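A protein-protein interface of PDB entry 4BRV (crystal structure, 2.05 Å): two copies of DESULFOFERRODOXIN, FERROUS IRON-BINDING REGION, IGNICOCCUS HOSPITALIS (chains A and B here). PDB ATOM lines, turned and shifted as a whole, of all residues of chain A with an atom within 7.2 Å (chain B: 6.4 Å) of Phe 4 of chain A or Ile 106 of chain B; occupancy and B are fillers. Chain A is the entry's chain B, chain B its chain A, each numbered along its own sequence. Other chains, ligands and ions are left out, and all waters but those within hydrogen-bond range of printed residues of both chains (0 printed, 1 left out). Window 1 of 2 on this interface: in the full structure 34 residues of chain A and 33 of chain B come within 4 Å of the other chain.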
ATOM      1  N   MET A   1      -0.619   3.999  -4.990  1.00  0.00           N
ATOM      2  CA  MET A   1      -0.718   2.849  -4.103  1.00  0.00           C
ATOM      3  C   MET A   1       0.664   2.279  -3.870  1.00  0.00           C
ATOM      4  O   MET A   1       1.652   2.791  -4.403  1.00  0.00           O
ATOM      5  CB  MET A   1      -1.619   1.773  -4.710  1.00  0.00           C
ATOM      6  CG  MET A   1      -1.171   1.306  -6.084  1.00  0.00           C
ATOM      7  SD  MET A   1      -2.476   0.456  -6.994  1.00  0.00           S
ATOM      8  CE  MET A   1      -2.374   1.269  -8.588  1.00  0.00           C
ATOM      9  N   LYS A   2       0.724   1.210  -3.082  1.00  0.00           N
ATOM     10  CA  LYS A   2       1.993   0.569  -2.754  1.00  0.00           C
ATOM     11  C   LYS A   2       2.486  -0.349  -3.867  1.00  0.00           C
ATOM     12  O   LYS A   2       1.706  -1.114  -4.449  1.00  0.00           O
ATOM     13  CB  LYS A   2       1.872  -0.225  -1.451  1.00  0.00           C
ATOM     14  CG  LYS A   2       1.951   0.624  -0.198  1.00  0.00           C
ATOM     15  CD  LYS A   2       2.571  -0.158   0.947  1.00  0.00           C
ATOM     16  CE  LYS A   2       3.289   0.766   1.930  1.00  0.00           C
ATOM     17  NZ  LYS A   2       3.983   0.014   3.026  1.00  0.00           N
ATOM     18  N   SER A   3       3.784  -0.273  -4.155  1.00  0.00           N
ATOM     19  CA  SER A   3       4.417  -1.211  -5.072  1.00  0.00           C
ATOM     20  C   SER A   3       4.626  -2.528  -4.344  1.00  0.00           C
ATOM     21  O   SER A   3       4.626  -2.572  -3.111  1.00  0.00           O
ATOM     22  CB  SER A   3       5.761  -0.676  -5.554  1.00  0.00           C
ATOM     23  OG  SER A   3       6.660  -0.579  -4.469  1.00  0.00           O
ATOM     24  N   PHE A   4       4.781  -3.603  -5.107  1.00  0.00           N
ATOM     25  CA  PHE A   4       4.966  -4.925  -4.531  1.00  0.00           C
ATOM     26  C   PHE A   4       6.153  -4.975  -3.552  1.00  0.00           C
ATOM     27  O   PHE A   4       6.062  -5.589  -2.479  1.00  0.00           O
ATOM     28  CB  PHE A   4       5.167  -5.950  -5.648  1.00  0.00           C
ATOM     29  CG  PHE A   4       5.349  -7.341  -5.148  1.00  0.00           C
ATOM     30  CD1 PHE A   4       4.266  -8.064  -4.680  1.00  0.00           C
ATOM     31  CD2 PHE A   4       6.606  -7.933  -5.135  1.00  0.00           C
ATOM     32  CE1 PHE A   4       4.427  -9.351  -4.196  1.00  0.00           C
ATOM     33  CE2 PHE A   4       6.771  -9.227  -4.652  1.00  0.00           C
ATOM     34  CZ  PHE A   4       5.676  -9.932  -4.188  1.00  0.00           C
ATOM     35  N   GLY A   5       7.263  -4.332  -3.917  1.00  0.00           N
ATOM     36  CA  GLY A   5       8.468  -4.382  -3.098  1.00  0.00           C
ATOM     37  C   GLY A   5       8.314  -3.767  -1.711  1.00  0.00           C
ATOM     38  O   GLY A   5       9.014  -4.156  -0.759  1.00  0.00           O
ATOM     39  N   GLU A   6       7.396  -2.810  -1.580  1.00  0.00           N
ATOM     40  CA  GLU A   6       7.148  -2.197  -0.284  1.00  0.00           C
ATOM     41  C   GLU A   6       6.406  -3.142   0.662  1.00  0.00           C
ATOM     42  O   GLU A   6       6.314  -2.868   1.860  1.00  0.00           O
ATOM     43  CB  GLU A   6       6.346  -0.905  -0.433  1.00  0.00           C
ATOM     44  CG  GLU A   6       6.987   0.165  -1.307  1.00  0.00           C
ATOM     45  CD  GLU A   6       6.010   1.283  -1.642  1.00  0.00           C
ATOM     46  OE1 GLU A   6       5.108   1.552  -0.815  1.00  0.00           O
ATOM     47  OE2 GLU A   6       6.132   1.884  -2.731  1.00  0.00           O
ATOM     48  N   LEU A   7       5.872  -4.243   0.128  1.00  0.00           N
ATOM     49  CA  LEU A   7       4.997  -5.125   0.908  1.00  0.00           C
ATOM     50  C   LEU A   7       5.784  -6.198   1.662  1.00  0.00           C
ATOM     51  O   LEU A   7       5.304  -6.774   2.647  1.00  0.00           O
ATOM     52  CB  LEU A   7       3.938  -5.781   0.015  1.00  0.00           C
ATOM     53  CG  LEU A   7       3.012  -4.830  -0.736  1.00  0.00           C
ATOM     54  CD1 LEU A   7       1.911  -5.612  -1.462  1.00  0.00           C
ATOM     55  CD2 LEU A   7       2.405  -3.842   0.234  1.00  0.00           C
ATOM     56  N   ILE A   8       6.996  -6.456   1.199  1.00  0.00           N
ATOM     57  CA  ILE A   8       7.803  -7.519   1.764  1.00  0.00           C
ATOM     58  C   ILE A   8       8.290  -7.099   3.141  1.00  0.00           C
ATOM     59  O   ILE A   8       8.833  -6.002   3.305  1.00  0.00           O
ATOM     60  CB  ILE A   8       8.980  -7.833   0.851  1.00  0.00           C
ATOM     61  CG1 ILE A   8       8.453  -8.293  -0.519  1.00  0.00           C
ATOM     62  CG2 ILE A   8       9.897  -8.888   1.484  1.00  0.00           C
ATOM     63  CD1 ILE A   8       9.561  -8.459  -1.557  1.00  0.00           C
ATOM     64  N   TRP A  60       6.776 -21.878   0.957  1.00  0.00           N
ATOM     65  CA  TRP A  60       7.938 -21.944   0.072  1.00  0.00           C
ATOM     66  C   TRP A  60       9.022 -20.953   0.428  1.00  0.00           C
ATOM     67  O   TRP A  60       8.792 -20.010   1.204  1.00  0.00           O
ATOM     68  CB  TRP A  60       7.533 -21.765  -1.405  1.00  0.00           C
ATOM     69  CG  TRP A  60       6.706 -20.554  -1.734  1.00  0.00           C
ATOM     70  CD1 TRP A  60       5.362 -20.534  -2.015  1.00  0.00           C
ATOM     71  CD2 TRP A  60       7.164 -19.198  -1.887  1.00  0.00           C
ATOM     72  NE1 TRP A  60       4.960 -19.253  -2.315  1.00  0.00           N
ATOM     73  CE2 TRP A  60       6.041 -18.417  -2.245  1.00  0.00           C
ATOM     74  CE3 TRP A  60       8.407 -18.570  -1.747  1.00  0.00           C
ATOM     75  CZ2 TRP A  60       6.129 -17.041  -2.465  1.00  0.00           C
ATOM     76  CZ3 TRP A  60       8.494 -17.214  -1.958  1.00  0.00           C
ATOM     77  CH2 TRP A  60       7.366 -16.458  -2.322  1.00  0.00           C
ATOM     78  N   TYR A  64      17.520 -15.580  -4.135  1.00  0.00           N
ATOM     79  CA  TYR A  64      18.000 -14.746  -5.232  1.00  0.00           C
ATOM     80  C   TYR A  64      19.404 -14.282  -4.881  1.00  0.00           C
ATOM     81  O   TYR A  64      19.802 -14.333  -3.709  1.00  0.00           O
ATOM     82  CB  TYR A  64      17.106 -13.533  -5.407  1.00  0.00           C
ATOM     83  CG  TYR A  64      15.692 -13.844  -5.855  1.00  0.00           C
ATOM     84  CD1 TYR A  64      14.722 -14.236  -4.943  1.00  0.00           C
ATOM     85  CD2 TYR A  64      15.325 -13.720  -7.194  1.00  0.00           C
ATOM     86  CE1 TYR A  64      13.409 -14.502  -5.357  1.00  0.00           C
ATOM     87  CE2 TYR A  64      14.032 -13.989  -7.619  1.00  0.00           C
ATOM     88  CZ  TYR A  64      13.082 -14.372  -6.692  1.00  0.00           C
ATOM     89  OH  TYR A  64      11.805 -14.622  -7.119  1.00  0.00           O
ATOM     90  N   ILE A 106      13.689 -15.406   0.524  1.00  0.00           N
ATOM     91  CA  ILE A 106      12.332 -14.910   0.730  1.00  0.00           C
ATOM     92  C   ILE A 106      11.452 -16.093   1.077  1.00  0.00           C
ATOM     93  O   ILE A 106      11.395 -17.058   0.310  1.00  0.00           O
ATOM     94  CB  ILE A 106      11.753 -14.314  -0.560  1.00  0.00           C
ATOM     95  CG1 ILE A 106      12.752 -13.356  -1.218  1.00  0.00           C
ATOM     96  CG2 ILE A 106      10.388 -13.667  -0.271  1.00  0.00           C
ATOM     97  CD1 ILE A 106      12.905 -12.050  -0.482  1.00  0.00           C
ATOM     98  N   LEU A 114       5.234 -12.218   3.178  1.00  0.00           N
ATOM     99  CA  LEU A 114       6.532 -12.462   2.573  1.00  0.00           C
ATOM    100  C   LEU A 114       7.589 -11.830   3.439  1.00  0.00           C
ATOM    101  O   LEU A 114       7.463 -10.658   3.807  1.00  0.00           O
ATOM    102  CB  LEU A 114       6.577 -11.806   1.191  1.00  0.00           C
ATOM    103  CG  LEU A 114       5.718 -12.472   0.117  1.00  0.00           C
ATOM    104  CD1 LEU A 114       5.448 -11.506  -0.997  1.00  0.00           C
ATOM    105  CD2 LEU A 114       6.444 -13.677  -0.423  1.00  0.00           C
ATOM    106  N   PHE B   4      15.634  -6.534  -1.041  1.00  0.00           N
ATOM    107  CA  PHE B   4      15.128  -7.229  -2.219  1.00  0.00           C
ATOM    108  C   PHE B   4      14.028  -6.431  -2.933  1.00  0.00           C
ATOM    109  O   PHE B   4      13.984  -6.378  -4.167  1.00  0.00           O
ATOM    110  CB  PHE B   4      14.603  -8.606  -1.812  1.00  0.00           C
ATOM    111  CG  PHE B   4      14.027  -9.383  -2.946  1.00  0.00           C
ATOM    112  CD1 PHE B   4      14.860 -10.058  -3.833  1.00  0.00           C
ATOM    113  CD2 PHE B   4      12.652  -9.447  -3.139  1.00  0.00           C
ATOM    114  CE1 PHE B   4      14.332 -10.777  -4.892  1.00  0.00           C
ATOM    115  CE2 PHE B   4      12.117 -10.166  -4.213  1.00  0.00           C
ATOM    116  CZ  PHE B   4      12.963 -10.835  -5.078  1.00  0.00           C
ATOM    117  N   GLY B   5      13.143  -5.802  -2.161  1.00  0.00           N
ATOM    118  CA  GLY B   5      12.021  -5.094  -2.759  1.00  0.00           C
ATOM    119  C   GLY B   5      12.448  -3.931  -3.640  1.00  0.00           C
ATOM    120  O   GLY B   5      11.723  -3.528  -4.559  1.00  0.00           O
ATOM    121  N   ILE B   8      13.203  -4.789  -7.634  1.00  0.00           N
ATOM    122  CA  ILE B   8      12.170  -5.096  -8.616  1.00  0.00           C
ATOM    123  C   ILE B   8      11.943  -3.896  -9.524  1.00  0.00           C
ATOM    124  O   ILE B   8      11.727  -2.782  -9.046  1.00  0.00           O
ATOM    125  CB  ILE B   8      10.867  -5.506  -7.913  1.00  0.00           C
ATOM    126  CG1 ILE B   8      11.109  -6.764  -7.061  1.00  0.00           C
ATOM    127  CG2 ILE B   8       9.733  -5.737  -8.912  1.00  0.00           C
ATOM    128  CD1 ILE B   8       9.908  -7.116  -6.158  1.00  0.00           C
ATOM    129  N   THR B  10      10.003  -1.424 -12.014  1.00  0.00           N
ATOM    130  CA  THR B  10       8.689  -0.921 -12.371  1.00  0.00           C
ATOM    131  C   THR B  10       8.976   0.133 -13.427  1.00  0.00           C
ATOM    132  O   THR B  10      10.079   0.680 -13.455  1.00  0.00           O
ATOM    133  CB  THR B  10       7.975  -0.318 -11.148  1.00  0.00           C
ATOM    134  OG1 THR B  10       8.644   0.879 -10.743  1.00  0.00           O
ATOM    135  CG2 THR B  10       8.011  -1.297  -9.983  1.00  0.00           C
ATOM    136  N   ARG B  13       9.833   3.735 -12.180  1.00  0.00           N
ATOM    137  CA  ARG B  13      11.075   3.849 -11.419  1.00  0.00           C
ATOM    138  C   ARG B  13      12.300   3.407 -12.212  1.00  0.00           C
ATOM    139  O   ARG B  13      13.398   3.324 -11.662  1.00  0.00           O
ATOM    140  CB  ARG B  13      10.993   3.049 -10.113  1.00  0.00           C
ATOM    141  CG  ARG B  13       9.986   3.588  -9.106  1.00  0.00           C
ATOM    142  CD  ARG B  13      10.293   3.122  -7.683  1.00  0.00           C
ATOM    143  NE  ARG B  13      10.115   1.683  -7.497  1.00  0.00           N
ATOM    144  CZ  ARG B  13       8.959   1.107  -7.177  1.00  0.00           C
ATOM    145  NH1 ARG B  13       7.867   1.844  -7.017  1.00  0.00           N
ATOM    146  NH2 ARG B  13       8.890  -0.209  -7.023  1.00  0.00           N
ATOM    147  N   PRO B  27       4.710  -6.935 -17.215  1.00  0.00           N
ATOM    148  CA  PRO B  27       3.505  -7.731 -17.459  1.00  0.00           C
ATOM    149  C   PRO B  27       2.308  -6.849 -17.825  1.00  0.00           C
ATOM    150  O   PRO B  27       2.171  -5.737 -17.299  1.00  0.00           O
ATOM    151  CB  PRO B  27       3.250  -8.397 -16.101  1.00  0.00           C
ATOM    152  CG  PRO B  27       4.617  -8.427 -15.428  1.00  0.00           C
ATOM    153  CD  PRO B  27       5.254  -7.139 -15.857  1.00  0.00           C
ATOM    154  N   TRP B  60       8.959 -17.252 -15.733  1.00  0.00           N
ATOM    155  CA  TRP B  60       7.776 -17.445 -14.899  1.00  0.00           C
ATOM    156  C   TRP B  60       7.046 -16.154 -14.568  1.00  0.00           C
ATOM    157  O   TRP B  60       7.582 -15.047 -14.743  1.00  0.00           O
ATOM    158  CB  TRP B  60       8.111 -18.224 -13.612  1.00  0.00           C
ATOM    159  CG  TRP B  60       9.230 -17.678 -12.755  1.00  0.00           C
ATOM    160  CD1 TRP B  60      10.502 -18.187 -12.640  1.00  0.00           C
ATOM    161  CD2 TRP B  60       9.156 -16.573 -11.838  1.00  0.00           C
ATOM    162  NE1 TRP B  60      11.221 -17.458 -11.710  1.00  0.00           N
ATOM    163  CE2 TRP B  60      10.423 -16.459 -11.215  1.00  0.00           C
ATOM    164  CE3 TRP B  60       8.149 -15.660 -11.497  1.00  0.00           C
ATOM    165  CZ2 TRP B  60      10.708 -15.463 -10.271  1.00  0.00           C
ATOM    166  CZ3 TRP B  60       8.426 -14.676 -10.556  1.00  0.00           C
ATOM    167  CH2 TRP B  60       9.696 -14.587  -9.951  1.00  0.00           C
ATOM    168  N   ILE B  61       5.796 -16.307 -14.140  1.00  0.00           N
ATOM    169  CA  ILE B  61       4.996 -15.184 -13.669  1.00  0.00           C
ATOM    170  C   ILE B  61       4.324 -15.601 -12.369  1.00  0.00           C
ATOM    171  O   ILE B  61       3.840 -16.741 -12.252  1.00  0.00           O
ATOM    172  CB  ILE B  61       3.914 -14.821 -14.678  1.00  0.00           C
ATOM    173  CG1 ILE B  61       4.547 -14.186 -15.910  1.00  0.00           C
ATOM    174  CG2 ILE B  61       2.901 -13.865 -14.073  1.00  0.00           C
ATOM    175  CD1 ILE B  61       3.568 -13.984 -17.043  1.00  0.00           C
ATOM    176  N   GLU B  62       4.341 -14.704 -11.383  1.00  0.00           N
ATOM    177  CA  GLU B  62       3.652 -14.925 -10.107  1.00  0.00           C
ATOM    178  C   GLU B  62       2.596 -13.842  -9.965  1.00  0.00           C
ATOM    179  O   GLU B  62       2.827 -12.691 -10.385  1.00  0.00           O
ATOM    180  CB  GLU B  62       4.655 -14.827  -8.951  1.00  0.00           C
ATOM    181  CG  GLU B  62       5.603 -16.009  -8.855  1.00  0.00           C
ATOM    182  CD  GLU B  62       6.585 -15.890  -7.706  1.00  0.00           C
ATOM    183  OE1 GLU B  62       6.723 -14.788  -7.139  1.00  0.00           O
ATOM    184  OE2 GLU B  62       7.235 -16.905  -7.373  1.00  0.00           O
ATOM    185  N   LEU B  63       1.455 -14.197  -9.376  1.00  0.00           N
ATOM    186  CA  LEU B  63       0.375 -13.250  -9.119  1.00  0.00           C
ATOM    187  C   LEU B  63       0.139 -13.165  -7.626  1.00  0.00           C
ATOM    188  O   LEU B  63       0.022 -14.197  -6.963  1.00  0.00           O
ATOM    189  CB  LEU B  63      -0.937 -13.767  -9.704  1.00  0.00           C
ATOM    190  CG  LEU B  63      -1.306 -13.602 -11.165  1.00  0.00           C
ATOM    191  CD1 LEU B  63      -2.812 -13.667 -11.255  1.00  0.00           C
ATOM    192  CD2 LEU B  63      -0.793 -12.290 -11.683  1.00  0.00           C
ATOM    193  N   TYR B  64      -0.004 -11.949  -7.110  1.00  0.00           N
ATOM    194  CA  TYR B  64      -0.276 -11.731  -5.697  1.00  0.00           C
ATOM    195  C   TYR B  64      -1.456 -10.780  -5.606  1.00  0.00           C
ATOM    196  O   TYR B  64      -1.751 -10.072  -6.578  1.00  0.00           O
ATOM    197  CB  TYR B  64       0.917 -11.071  -5.029  1.00  0.00           C
ATOM    198  CG  TYR B  64       2.148 -11.952  -4.926  1.00  0.00           C
ATOM    199  CD1 TYR B  64       3.054 -12.032  -5.967  1.00  0.00           C
ATOM    200  CD2 TYR B  64       2.409 -12.684  -3.764  1.00  0.00           C
ATOM    201  CE1 TYR B  64       4.217 -12.829  -5.859  1.00  0.00           C
ATOM    202  CE2 TYR B  64       3.535 -13.486  -3.655  1.00  0.00           C
ATOM    203  CZ  TYR B  64       4.435 -13.549  -4.698  1.00  0.00           C
ATOM    204  OH  TYR B  64       5.554 -14.344  -4.570  1.00  0.00           O
ATOM    205  N   PRO B  74       1.003  -9.599   1.042  1.00  0.00           N
ATOM    206  CA  PRO B  74      -0.174  -9.927   0.235  1.00  0.00           C
ATOM    207  C   PRO B  74      -0.454 -11.416   0.292  1.00  0.00           C
ATOM    208  O   PRO B  74       0.214 -12.180   1.004  1.00  0.00           O
ATOM    209  CB  PRO B  74       0.269  -9.549  -1.173  1.00  0.00           C
ATOM    210  CG  PRO B  74       1.765  -9.950  -1.176  1.00  0.00           C
ATOM    211  CD  PRO B  74       2.256  -9.751   0.271  1.00  0.00           C
ATOM    212  N   TYR B 104      -1.228  -7.928  -8.274  1.00  0.00           N
ATOM    213  CA  TYR B 104       0.159  -7.719  -8.714  1.00  0.00           C
ATOM    214  C   TYR B 104       0.625  -8.879  -9.573  1.00  0.00           C
ATOM    215  O   TYR B 104       0.414 -10.040  -9.199  1.00  0.00           O
ATOM    216  CB  TYR B 104       1.123  -7.637  -7.515  1.00  0.00           C
ATOM    217  CG  TYR B 104       0.902  -6.462  -6.598  1.00  0.00           C
ATOM    218  CD1 TYR B 104       1.527  -5.246  -6.830  1.00  0.00           C
ATOM    219  CD2 TYR B 104       0.073  -6.568  -5.495  1.00  0.00           C
ATOM    220  CE1 TYR B 104       1.324  -4.169  -5.990  1.00  0.00           C
ATOM    221  CE2 TYR B 104      -0.134  -5.488  -4.648  1.00  0.00           C
ATOM    222  CZ  TYR B 104       0.491  -4.297  -4.904  1.00  0.00           C
ATOM    223  OH  TYR B 104       0.282  -3.220  -4.071  1.00  0.00           O
ATOM    224  N   ALA B 105       1.291  -8.575 -10.694  1.00  0.00           N
ATOM    225  CA  ALA B 105       1.942  -9.597 -11.517  1.00  0.00           C
ATOM    226  C   ALA B 105       3.444  -9.293 -11.574  1.00  0.00           C
ATOM    227  O   ALA B 105       3.846  -8.146 -11.841  1.00  0.00           O
ATOM    228  CB  ALA B 105       1.343  -9.618 -12.956  1.00  0.00           C
ATOM    229  N   ILE B 106       4.261 -10.319 -11.350  1.00  0.00           N
ATOM    230  CA  ILE B 106       5.707 -10.184 -11.342  1.00  0.00           C
ATOM    231  C   ILE B 106       6.207 -11.204 -12.333  1.00  0.00           C
ATOM    232  O   ILE B 106       5.879 -12.387 -12.209  1.00  0.00           O
ATOM    233  CB  ILE B 106       6.295 -10.590  -9.981  1.00  0.00           C
ATOM    234  CG1 ILE B 106       5.537  -9.922  -8.829  1.00  0.00           C
ATOM    235  CG2 ILE B 106       7.812 -10.326  -9.949  1.00  0.00           C
ATOM    236  CD1 ILE B 106       5.687  -8.443  -8.767  1.00  0.00           C
ATOM    237  N   SER B 107       6.962 -10.768 -13.336  1.00  0.00           N
ATOM    238  CA  SER B 107       7.494 -11.721 -14.294  1.00  0.00           C
ATOM    239  C   SER B 107       8.992 -11.718 -14.119  1.00  0.00           C
ATOM    240  O   SER B 107       9.542 -10.732 -13.604  1.00  0.00           O
ATOM    241  CB  SER B 107       7.127 -11.315 -15.714  1.00  0.00           C
ATOM    242  OG  SER B 107       7.711 -10.070 -16.027  1.00  0.00           O
ATOM    243  N   TYR B 108       9.650 -12.809 -14.516  1.00  0.00           N
ATOM    244  CA  TYR B 108      11.102 -12.913 -14.395  1.00  0.00           C
ATOM    245  C   TYR B 108      11.721 -13.280 -15.731  1.00  0.00           C
ATOM    246  O   TYR B 108      11.325 -14.268 -16.367  1.00  0.00           O
ATOM    247  CB  TYR B 108      11.488 -13.950 -13.326  1.00  0.00           C
ATOM    248  CG  TYR B 108      12.984 -14.251 -13.237  1.00  0.00           C
ATOM    249  CD1 TYR B 108      13.837 -13.405 -12.546  1.00  0.00           C
ATOM    250  CD2 TYR B 108      13.530 -15.401 -13.815  1.00  0.00           C
ATOM    251  CE1 TYR B 108      15.221 -13.675 -12.441  1.00  0.00           C
ATOM    252  CE2 TYR B 108      14.916 -15.694 -13.711  1.00  0.00           C
ATOM    253  CZ  TYR B 108      15.746 -14.816 -13.018  1.00  0.00           C
ATOM    254  OH  TYR B 108      17.101 -15.065 -12.897  1.00  0.00           O
ATOM    255  N   LEU B 114      13.407  -8.877 -12.477  1.00  0.00           N
ATOM    256  CA  LEU B 114      12.018  -8.993 -12.044  1.00  0.00           C
ATOM    257  C   LEU B 114      11.262  -7.726 -12.379  1.00  0.00           C
ATOM    258  O   LEU B 114      11.725  -6.629 -12.073  1.00  0.00           O
ATOM    259  CB  LEU B 114      11.974  -9.196 -10.525  1.00  0.00           C
ATOM    260  CG  LEU B 114      12.531 -10.512 -10.008  1.00  0.00           C
ATOM    261  CD1 LEU B 114      12.893 -10.382  -8.545  1.00  0.00           C
ATOM    262  CD2 LEU B 114      11.464 -11.558 -10.177  1.00  0.00           C
ATOM    263  N   TRP B 115      10.085  -7.870 -12.985  1.00  0.00           N
ATOM    264  CA  TRP B 115       9.294  -6.709 -13.375  1.00  0.00           C
ATOM    265  C   TRP B 115       7.887  -6.789 -12.804  1.00  0.00           C
ATOM    266  O   TRP B 115       7.277  -7.869 -12.763  1.00  0.00           O
ATOM    267  CB  TRP B 115       9.235  -6.608 -14.894  1.00  0.00           C
ATOM    268  CG  TRP B 115      10.573  -6.228 -15.459  1.00  0.00           C
ATOM    269  CD1 TRP B 115      11.656  -7.047 -15.637  1.00  0.00           C
ATOM    270  CD2 TRP B 115      10.978  -4.921 -15.879  1.00  0.00           C
ATOM    271  NE1 TRP B 115      12.717  -6.317 -16.153  1.00  0.00           N
ATOM    272  CE2 TRP B 115      12.320  -5.013 -16.309  1.00  0.00           C
ATOM    273  CE3 TRP B 115      10.336  -3.681 -15.931  1.00  0.00           C
ATOM    274  CZ2 TRP B 115      13.025  -3.905 -16.785  1.00  0.00           C
ATOM    275  CZ3 TRP B 115      11.030  -2.591 -16.401  1.00  0.00           C
ATOM    276  CH2 TRP B 115      12.364  -2.705 -16.831  1.00  0.00           C
ATOM    277  N   GLU B 116       7.359  -5.640 -12.399  1.00  0.00           N
ATOM    278  CA  GLU B 116       6.077  -5.594 -11.706  1.00  0.00           C
ATOM    279  C   GLU B 116       4.997  -4.797 -12.449  1.00  0.00           C
ATOM    280  O   GLU B 116       5.256  -3.711 -12.993  1.00  0.00           O
ATOM    281  CB  GLU B 116       6.276  -4.985 -10.316  1.00  0.00           C
ATOM    282  CG  GLU B 116       4.976  -4.783  -9.540  1.00  0.00           C
ATOM    283  CD  GLU B 116       5.101  -3.728  -8.460  1.00  0.00           C
ATOM    284  OE1 GLU B 116       6.226  -3.455  -8.013  1.00  0.00           O
ATOM    285  OE2 GLU B 116       4.074  -3.164  -8.052  1.00  0.00           O
ATOM    286  N   ALA B 117       3.778  -5.329 -12.476  1.00  0.00           N
ATOM    287  CA  ALA B 117       2.642  -4.526 -12.891  1.00  0.00           C
ATOM    288  C   ALA B 117       1.557  -4.679 -11.837  1.00  0.00           C
ATOM    289  O   ALA B 117       1.517  -5.685 -11.095  1.00  0.00           O
ATOM    290  CB  ALA B 117       2.128  -4.948 -14.265  1.00  0.00           C
ATOM    291  N   ARG B 118       0.671  -3.698 -11.752  1.00  0.00           N
ATOM    292  CA  ARG B 118      -0.357  -3.803 -10.730  1.00  0.00           C
ATOM    293  C   ARG B 118      -1.676  -3.290 -11.262  1.00  0.00           C
ATOM    294  O   ARG B 118      -1.686  -2.417 -12.117  1.00  0.00           O
ATOM    295  CB  ARG B 118       0.075  -3.031  -9.481  1.00  0.00           C
ATOM    296  CG  ARG B 118      -0.101  -1.520  -9.581  1.00  0.00           C
ATOM    297  CD  ARG B 118       0.709  -0.797  -8.504  1.00  0.00           C
ATOM    298  NE  ARG B 118       2.128  -1.141  -8.608  1.00  0.00           N
ATOM    299  CZ  ARG B 118       3.121  -0.263  -8.511  1.00  0.00           C
ATOM    300  NH1 ARG B 118       2.857   1.018  -8.291  1.00  0.00           N
ATOM    301  NH2 ARG B 118       4.377  -0.668  -8.627  1.00  0.00           N
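Among the printed residues, pairs that only touch across the chains: Met 1 of chain A with Arg 118 of chain B (3.7 Å), Ser 3 of chain A with Glu 116 of chain B (3.6 Å), Ser 3 of chain A with Arg 118 of chain B (3.4 Å), Phe 4 of chain A with Ile 8 of chain B (3.6 Å), Phe 4 of chain A with Tyr 64 of chain B (3.5 Å), Phe 4 of chain A with Tyr 104 of chain B (3.6 Å), Phe 4 of chain A with Ile 106 of chain B (3.8 Å), Gly 5 of chain A with Gly 5 of chain B (3.6 Å), Leu 7 of chain A with Tyr 104 of chain B (3.8 Å), Ile 8 of chain A with Phe 4 of chain B (3.6 Å), Trp 60 of chain A with Tyr 64 of chain B (3.5 Å), Tyr 64 of chain A with Phe 4 of chain B (3.5 Å), Tyr 64 of chain A with Trp 60 of chain B (3.4 Å), Tyr 64 of chain A with Leu 114 of chain B (3.9 Å), Ile 106 of chain A with Phe 4 of chain B (3.7 Å), Leu 114 of chain A with Tyr 64 of chain B (3.8 Å) and Leu 114 of chain A with Pro 74 of chain B (3.9 Å).
Phe 4 of chain A touches Ile 8 of chain B, and with the chains exchanged Ile 8 of chain A touches Phe 4 of chain B. Gly 5 of chain A touches its own counterpart, Gly 5 of chain B. Trp 60 of chain A touches Tyr 64 of chain B, and with the chains exchanged Tyr 64 of chain A touches Trp 60 of chain B. Tyr 64 of chain A touches Leu 114 of chain B, and with the chains exchanged Leu 114 of chain A touches Tyr 64 of chain B. Of the 20 pairs that touch across the chains among the printed residues, 11 have their exchanged pair printed and touching as well.
Phe 4 of chain A touches five residues of chain B. Printed residues of chain A within 4 Å of Ile 106 of chain B: Phe 4 (3.8 Å). Of the printed residues of chain A, Gly 5 of chain B touches Gly 5. Of the printed residues of chain A, Arg 118 of chain B touches Met 1 and Ser 3. Printed residues of chain A within 4 Å of Ile 8 of chain B: Phe 4 (3.6 Å). Of the printed residues of chain A, Arg 13 of chain B touches Ser 3. Of the printed residues of chain B, Lys 2 of chain A touches Tyr 104. The nearest residue of chain B that does not touch Phe 4 of chain A is Pro 74 of chain B (4.1 Å). The nearest residue of chain A that does not touch Ile 106 of chain B is Tyr 64 of chain A (6.5 Å).
Of the 22 printed residues of chain B, 12 touch a printed residue of chain A. Hydrophobic or aromatic side chains of chain A within 4 Å of the printed part of chain B: Met 1, Phe 4, Leu 7, Ile 8, Trp 60, Tyr 64, Ile 106 and Leu 114. Among the printed residues, 20 pairs touch across the chains.
The guanidinium group (NH2) of Arg 13 of chain B sits at hydrogen-bond distance from the side-chain hydroxyl (OG) of Ser 3 of chain A (3.4 Å). OE2 of Glu 116 of chain B lies within hydrogen-bond range of N of Phe 4 of chain A, at 3.1 Å. OH of Tyr 104 of chain B lies within hydrogen-bond range of O of Lys 2 of chain A, 2.6 Å away.
OE1 of Glu 62 of chain B lies within hydrogen-bond range of OH of Tyr 64 of chain B, 2.9 Å away. N of Glu 62 of chain B sits at hydrogen-bond distance from O of Ile 106 of chain B, at 2.9 Å. The side-chain hydroxyl of Thr 10 of chain B sits close to the backbone NH of Arg 13 of chain B (3.4 Å). The side-chain carboxylate (OE2) of Glu 116 of chain B lies within salt-bridge range of the guanidinium group (NH2) of Arg 118 of chain B (2.6 Å). The backbone carbonyl oxygen (O) of Tyr 64 of chain B lies within hydrogen-bond range of the backbone NH (N) of Tyr 104 of chain B. The side-chain hydroxyl of Ser 3 of chain A sits at hydrogen-bond distance from the side-chain carboxylate of Glu 6 of chain A (3.1 Å).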
